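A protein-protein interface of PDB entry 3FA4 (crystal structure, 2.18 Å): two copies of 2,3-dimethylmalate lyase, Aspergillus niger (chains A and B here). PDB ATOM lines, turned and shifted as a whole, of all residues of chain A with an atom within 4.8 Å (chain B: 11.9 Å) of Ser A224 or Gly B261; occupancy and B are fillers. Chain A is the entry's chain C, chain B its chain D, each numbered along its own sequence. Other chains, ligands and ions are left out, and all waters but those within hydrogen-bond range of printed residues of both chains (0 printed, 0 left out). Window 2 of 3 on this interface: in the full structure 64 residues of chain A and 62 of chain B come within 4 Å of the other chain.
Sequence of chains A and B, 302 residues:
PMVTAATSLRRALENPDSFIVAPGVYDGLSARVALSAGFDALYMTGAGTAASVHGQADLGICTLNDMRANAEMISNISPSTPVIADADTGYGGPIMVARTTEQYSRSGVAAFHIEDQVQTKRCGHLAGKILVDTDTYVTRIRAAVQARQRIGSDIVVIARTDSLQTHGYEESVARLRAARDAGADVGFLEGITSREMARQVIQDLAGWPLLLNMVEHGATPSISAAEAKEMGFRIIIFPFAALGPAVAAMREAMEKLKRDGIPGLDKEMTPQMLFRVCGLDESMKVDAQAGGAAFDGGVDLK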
ATOM      1  N   SER A 222       0.357   9.755  11.167  1.00  0.00           N
ATOM      2  CA  SER A 222       0.564  10.847  12.091  1.00  0.00           C
ATOM      3  C   SER A 222       1.658  10.516  13.073  1.00  0.00           C
ATOM      4  O   SER A 222       1.541   9.576  13.834  1.00  0.00           O
ATOM      5  CB  SER A 222      -0.746  11.269  12.753  1.00  0.00           C
ATOM      6  OG  SER A 222      -1.552  11.883  11.737  1.00  0.00           O
ATOM      7  N   ILE A 223       2.753  11.230  12.999  1.00  0.00           N
ATOM      8  CA  ILE A 223       3.873  11.019  13.919  1.00  0.00           C
ATOM      9  C   ILE A 223       4.059  12.297  14.746  1.00  0.00           C
ATOM     10  O   ILE A 223       4.135  13.406  14.219  1.00  0.00           O
ATOM     11  CB  ILE A 223       5.167  10.557  13.185  1.00  0.00           C
ATOM     12  CG1 ILE A 223       4.948   9.208  12.509  1.00  0.00           C
ATOM     13  CG2 ILE A 223       6.334  10.450  14.136  1.00  0.00           C
ATOM     14  CD1 ILE A 223       5.799   9.026  11.292  1.00  0.00           C
ATOM     15  N   SER A 224       4.040  12.135  16.051  1.00  0.00           N
ATOM     16  CA  SER A 224       4.082  13.260  16.935  1.00  0.00           C
ATOM     17  C   SER A 224       5.573  13.608  17.165  1.00  0.00           C
ATOM     18  O   SER A 224       6.439  12.766  16.940  1.00  0.00           O
ATOM     19  CB  SER A 224       3.434  12.807  18.247  1.00  0.00           C
ATOM     20  OG  SER A 224       4.268  11.843  18.857  1.00  0.00           O
ATOM     21  N   ALA A 225       5.877  14.814  17.613  1.00  0.00           N
ATOM     22  CA  ALA A 225       7.258  15.136  17.922  1.00  0.00           C
ATOM     23  C   ALA A 225       8.027  14.044  18.697  1.00  0.00           C
ATOM     24  O   ALA A 225       9.152  13.732  18.319  1.00  0.00           O
ATOM     25  CB  ALA A 225       7.336  16.455  18.665  1.00  0.00           C
ATOM     26  N   ALA A 226       7.433  13.471  19.753  1.00  0.00           N
ATOM     27  CA  ALA A 226       8.113  12.468  20.641  1.00  0.00           C
ATOM     28  C   ALA A 226       8.393  11.128  19.953  1.00  0.00           C
ATOM     29  O   ALA A 226       9.477  10.547  20.081  1.00  0.00           O
ATOM     30  CB  ALA A 226       7.307  12.222  21.955  1.00  0.00           C
ATOM     31  N   GLU A 227       7.386  10.604  19.263  1.00  0.00           N
ATOM     32  CA  GLU A 227       7.590   9.374  18.524  1.00  0.00           C
ATOM     33  C   GLU A 227       8.712   9.642  17.504  1.00  0.00           C
ATOM     34  O   GLU A 227       9.644   8.874  17.440  1.00  0.00           O
ATOM     35  CB  GLU A 227       6.285   8.911  17.867  1.00  0.00           C
ATOM     36  CG  GLU A 227       6.261   7.433  17.438  1.00  0.00           C
ATOM     37  CD  GLU A 227       5.038   7.156  16.551  1.00  0.00           C
ATOM     38  OE1 GLU A 227       4.015   7.848  16.763  1.00  0.00           O
ATOM     39  OE2 GLU A 227       5.084   6.277  15.659  1.00  0.00           O
ATOM     40  N   ALA A 228       8.653  10.767  16.769  1.00  0.00           N
ATOM     41  CA  ALA A 228       9.649  11.068  15.721  1.00  0.00           C
ATOM     42  C   ALA A 228      11.074  11.157  16.282  1.00  0.00           C
ATOM     43  O   ALA A 228      12.037  10.697  15.633  1.00  0.00           O
ATOM     44  CB  ALA A 228       9.281  12.336  14.935  1.00  0.00           C
ATOM     45  N   ILE A 236      11.479  17.982  13.270  1.00  0.00           N
ATOM     46  CA  ILE A 236      10.199  17.677  12.776  1.00  0.00           C
ATOM     47  C   ILE A 236       9.603  19.055  12.478  1.00  0.00           C
ATOM     48  O   ILE A 236       9.795  19.999  13.261  1.00  0.00           O
ATOM     49  CB  ILE A 236       9.374  16.880  13.774  1.00  0.00           C
ATOM     50  CG1 ILE A 236       7.998  16.600  13.175  1.00  0.00           C
ATOM     51  CG2 ILE A 236       9.169  17.725  15.037  1.00  0.00           C
ATOM     52  CD1 ILE A 236       7.246  15.579  13.954  1.00  0.00           C
ATOM     53  N   PHE A 238       5.979  21.189  10.968  1.00  0.00           N
ATOM     54  CA  PHE A 238       4.540  21.040  10.766  1.00  0.00           C
ATOM     55  C   PHE A 238       4.097  22.240   9.897  1.00  0.00           C
ATOM     56  O   PHE A 238       3.655  23.244  10.443  1.00  0.00           O
ATOM     57  CB  PHE A 238       3.747  21.047  12.078  1.00  0.00           C
ATOM     58  CG  PHE A 238       4.240  20.042  13.171  1.00  0.00           C
ATOM     59  CD1 PHE A 238       5.158  20.448  14.161  1.00  0.00           C
ATOM     60  CD2 PHE A 238       3.772  18.704  13.215  1.00  0.00           C
ATOM     61  CE1 PHE A 238       5.614  19.527  15.163  1.00  0.00           C
ATOM     62  CE2 PHE A 238       4.221  17.798  14.242  1.00  0.00           C
ATOM     63  CZ  PHE A 238       5.144  18.225  15.177  1.00  0.00           C
ATOM     64  N   GLU B 252      -4.475  29.226  19.706  1.00  0.00           N
ATOM     65  CA  GLU B 252      -5.071  28.049  20.217  1.00  0.00           C
ATOM     66  C   GLU B 252      -4.509  26.724  19.642  1.00  0.00           C
ATOM     67  O   GLU B 252      -4.339  25.751  20.394  1.00  0.00           O
ATOM     68  CB  GLU B 252      -6.557  28.178  19.958  1.00  0.00           C
ATOM     69  CG  GLU B 252      -7.378  27.381  20.937  1.00  0.00           C
ATOM     70  CD  GLU B 252      -8.621  28.114  21.409  1.00  0.00           C
ATOM     71  OE1 GLU B 252      -9.121  29.018  20.665  1.00  0.00           O
ATOM     72  OE2 GLU B 252      -9.068  27.760  22.536  1.00  0.00           O
ATOM     73  N   ALA B 253      -4.182  26.723  18.347  1.00  0.00           N
ATOM     74  CA  ALA B 253      -3.580  25.607  17.650  1.00  0.00           C
ATOM     75  C   ALA B 253      -2.120  25.465  18.037  1.00  0.00           C
ATOM     76  O   ALA B 253      -1.646  24.349  18.319  1.00  0.00           O
ATOM     77  CB  ALA B 253      -3.678  25.813  16.258  1.00  0.00           C
ATOM     78  N   MET B 254      -1.409  26.591  18.083  1.00  0.00           N
ATOM     79  CA  MET B 254      -0.053  26.595  18.615  1.00  0.00           C
ATOM     80  C   MET B 254      -0.004  26.028  20.042  1.00  0.00           C
ATOM     81  O   MET B 254       0.797  25.145  20.356  1.00  0.00           O
ATOM     82  CB  MET B 254       0.517  28.009  18.512  1.00  0.00           C
ATOM     83  CG  MET B 254       0.879  28.464  17.108  1.00  0.00           C
ATOM     84  SD  MET B 254       1.893  27.349  16.114  1.00  0.00           S
ATOM     85  CE  MET B 254       1.773  28.079  14.482  1.00  0.00           C
ATOM     86  N   GLU B 255      -0.881  26.468  20.928  1.00  0.00           N
ATOM     87  CA  GLU B 255      -0.752  25.972  22.329  1.00  0.00           C
ATOM     88  C   GLU B 255      -1.017  24.491  22.463  1.00  0.00           C
ATOM     89  O   GLU B 255      -0.415  23.836  23.312  1.00  0.00           O
ATOM     90  CB  GLU B 255      -1.603  26.781  23.345  1.00  0.00           C
ATOM     91  CG  GLU B 255      -1.222  28.272  23.352  1.00  0.00           C
ATOM     92  CD  GLU B 255      -2.292  29.158  23.973  1.00  0.00           C
ATOM     93  OE1 GLU B 255      -2.048  30.393  24.047  1.00  0.00           O
ATOM     94  OE2 GLU B 255      -3.376  28.633  24.364  1.00  0.00           O
ATOM     95  N   LYS B 256      -1.901  23.992  21.600  1.00  0.00           N
ATOM     96  CA  LYS B 256      -2.363  22.623  21.527  1.00  0.00           C
ATOM     97  C   LYS B 256      -1.317  21.647  20.969  1.00  0.00           C
ATOM     98  O   LYS B 256      -1.123  20.546  21.507  1.00  0.00           O
ATOM     99  CB  LYS B 256      -3.592  22.563  20.660  1.00  0.00           C
ATOM    100  CG  LYS B 256      -4.140  21.149  20.585  1.00  0.00           C
ATOM    101  CD  LYS B 256      -5.345  21.085  19.688  1.00  0.00           C
ATOM    102  CE  LYS B 256      -5.798  19.653  19.571  1.00  0.00           C
ATOM    103  NZ  LYS B 256      -6.714  19.681  18.421  1.00  0.00           N
ATOM    104  N   LEU B 257      -0.676  22.095  19.881  1.00  0.00           N
ATOM    105  CA  LEU B 257       0.571  21.549  19.335  1.00  0.00           C
ATOM    106  C   LEU B 257       1.731  21.510  20.366  1.00  0.00           C
ATOM    107  O   LEU B 257       2.509  20.504  20.482  1.00  0.00           O
ATOM    108  CB  LEU B 257       0.955  22.351  18.060  1.00  0.00           C
ATOM    109  CG  LEU B 257       2.353  22.017  17.571  1.00  0.00           C
ATOM    110  CD1 LEU B 257       2.469  20.540  17.260  1.00  0.00           C
ATOM    111  CD2 LEU B 257       2.638  22.909  16.369  1.00  0.00           C
ATOM    112  N   LYS B 258       1.856  22.566  21.154  1.00  0.00           N
ATOM    113  CA  LYS B 258       2.866  22.516  22.244  1.00  0.00           C
ATOM    114  C   LYS B 258       2.553  21.422  23.254  1.00  0.00           C
ATOM    115  O   LYS B 258       3.452  20.701  23.623  1.00  0.00           O
ATOM    116  CB  LYS B 258       3.097  23.896  22.923  1.00  0.00           C
ATOM    117  CG  LYS B 258       4.259  23.973  23.881  1.00  0.00           C
ATOM    118  CD  LYS B 258       5.555  24.350  23.169  1.00  0.00           C
ATOM    119  CE  LYS B 258       6.678  24.629  24.153  1.00  0.00           C
ATOM    120  NZ  LYS B 258       7.370  23.404  24.494  1.00  0.00           N
ATOM    121  N   ARG B 259       1.298  21.270  23.672  1.00  0.00           N
ATOM    122  CA  ARG B 259       0.926  20.236  24.659  1.00  0.00           C
ATOM    123  C   ARG B 259       0.984  18.853  24.039  1.00  0.00           C
ATOM    124  O   ARG B 259       1.487  17.888  24.686  1.00  0.00           O
ATOM    125  CB  ARG B 259      -0.476  20.436  25.280  1.00  0.00           C
ATOM    126  CG  ARG B 259      -0.665  21.626  26.253  1.00  0.00           C
ATOM    127  CD  ARG B 259      -2.159  21.793  26.732  1.00  0.00           C
ATOM    128  NE  ARG B 259      -3.185  21.545  25.695  1.00  0.00           N
ATOM    129  CZ  ARG B 259      -3.826  22.489  24.974  1.00  0.00           C
ATOM    130  NH1 ARG B 259      -3.613  23.774  25.157  1.00  0.00           N
ATOM    131  NH2 ARG B 259      -4.709  22.144  24.070  1.00  0.00           N
ATOM    132  N   ASP B 260       0.490  18.737  22.797  1.00  0.00           N
ATOM    133  CA  ASP B 260       0.272  17.414  22.199  1.00  0.00           C
ATOM    134  C   ASP B 260       1.379  16.842  21.314  1.00  0.00           C
ATOM    135  O   ASP B 260       1.442  15.629  21.087  1.00  0.00           O
ATOM    136  CB  ASP B 260      -1.021  17.413  21.423  1.00  0.00           C
ATOM    137  CG  ASP B 260      -2.235  17.574  22.308  1.00  0.00           C
ATOM    138  OD1 ASP B 260      -2.091  17.531  23.565  1.00  0.00           O
ATOM    139  OD2 ASP B 260      -3.345  17.718  21.723  1.00  0.00           O
ATOM    140  N   GLY B 261       2.238  17.705  20.792  1.00  0.00           N
ATOM    141  CA  GLY B 261       3.303  17.252  19.901  1.00  0.00           C
ATOM    142  C   GLY B 261       2.826  16.853  18.506  1.00  0.00           C
ATOM    143  O   GLY B 261       3.606  16.276  17.739  1.00  0.00           O
ATOM    144  N   ILE B 262       1.554  17.141  18.186  1.00  0.00           N
ATOM    145  CA  ILE B 262       1.017  16.932  16.838  1.00  0.00           C
ATOM    146  C   ILE B 262      -0.068  17.982  16.675  1.00  0.00           C
ATOM    147  O   ILE B 262      -0.733  18.212  17.647  1.00  0.00           O
ATOM    148  CB  ILE B 262       0.500  15.434  16.701  1.00  0.00           C
ATOM    149  CG1 ILE B 262       0.000  15.100  15.283  1.00  0.00           C
ATOM    150  CG2 ILE B 262      -0.518  15.059  17.790  1.00  0.00           C
ATOM    151  CD1 ILE B 262       1.060  14.763  14.315  1.00  0.00           C
ATOM    152  N   PRO B 263      -0.225  18.685  15.502  1.00  0.00           N
ATOM    153  CA  PRO B 263      -1.422  19.576  15.467  1.00  0.00           C
ATOM    154  C   PRO B 263      -2.788  18.958  15.869  1.00  0.00           C
ATOM    155  O   PRO B 263      -3.550  19.611  16.589  1.00  0.00           O
ATOM    156  CB  PRO B 263      -1.427  20.167  14.044  1.00  0.00           C
ATOM    157  CG  PRO B 263       0.009  20.042  13.562  1.00  0.00           C
ATOM    158  CD  PRO B 263       0.628  18.888  14.305  1.00  0.00           C
ATOM    159  N   GLY B 264      -3.087  17.732  15.429  1.00  0.00           N
ATOM    160  CA  GLY B 264      -4.446  17.193  15.519  1.00  0.00           C
ATOM    161  C   GLY B 264      -5.377  18.083  14.693  1.00  0.00           C
ATOM    162  O   GLY B 264      -6.482  18.415  15.143  1.00  0.00           O
ATOM    163  N   LEU B 265      -4.947  18.499  13.496  1.00  0.00           N
ATOM    164  CA  LEU B 265      -5.785  19.418  12.693  1.00  0.00           C
ATOM    165  C   LEU B 265      -6.979  18.665  12.146  1.00  0.00           C
ATOM    166  O   LEU B 265      -6.912  17.427  11.918  1.00  0.00           O
ATOM    167  CB  LEU B 265      -5.032  20.068  11.514  1.00  0.00           C
ATOM    168  CG  LEU B 265      -3.832  20.980  11.715  1.00  0.00           C
ATOM    169  CD1 LEU B 265      -3.348  21.585  10.414  1.00  0.00           C
ATOM    170  CD2 LEU B 265      -4.109  22.111  12.716  1.00  0.00           C
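The backbone carbonyl oxygen (O) of Gly B261 sits at hydrogen-bond distance from the backbone NH (N) of Ala A225 (2.7 Å).
OG of Ser A224 sits at hydrogen-bond distance from N of Glu A227.
Among the printed residues, pairs that only touch across the chains: Ile A223 with Ile B262, Ser A224 with Gly B261, Phe A238 with Leu B257, Phe A238 with Gly B261 and Phe A238 with Pro B263.
Of the printed residues of chain B, Ser A224 touches Gly B261 (3.2 Å). Gly B261 touches just these residues of chain A: Ser A224 (3.2 Å), Ala A225 (2.7 Å) and Phe A238 (3.6 Å). No residue of chain B comes within 4 Å of Ser A222. No residue of chain B comes within 4 Å of Ala A226. No residue of chain B comes within 4 Å of Glu A227. No residue of chain B comes within 4 Å of Ala A228. Printed residues of chain A within 4 Å of Leu B257: Phe A238 (3.9 Å). Printed residues of chain B within 4 Å of Phe A238: Leu B257 (3.9 Å), Gly B261 (3.6 Å) and Pro B263 (3.3 Å). Of the printed residues of chain A, Pro B263 touches Phe A238. Printed residues of chain A within 4 Å of Ile B262: Ile A223 (3.4 Å).
Of the 9 printed residues of chain A, 4 touch a printed residue of chain B. Hydrophobic or aromatic side chains of chain A within 4 Å of the printed part of chain B: Ala A225 and Phe A238. Of the 14 printed residues of chain B, 4 touch a printed residue of chain A. Printed residues of chain B that touch a printed residue of chain A: Leu B257, Gly B261, Ile B262 and Pro B263. Among the printed residues, 6 pairs touch across the chains. Among the printed residues, no Asp or Glu carboxylate lies within 4 Å of a Lys or Arg side-chain nitrogen of the other chain.
No position is printed for both chains.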
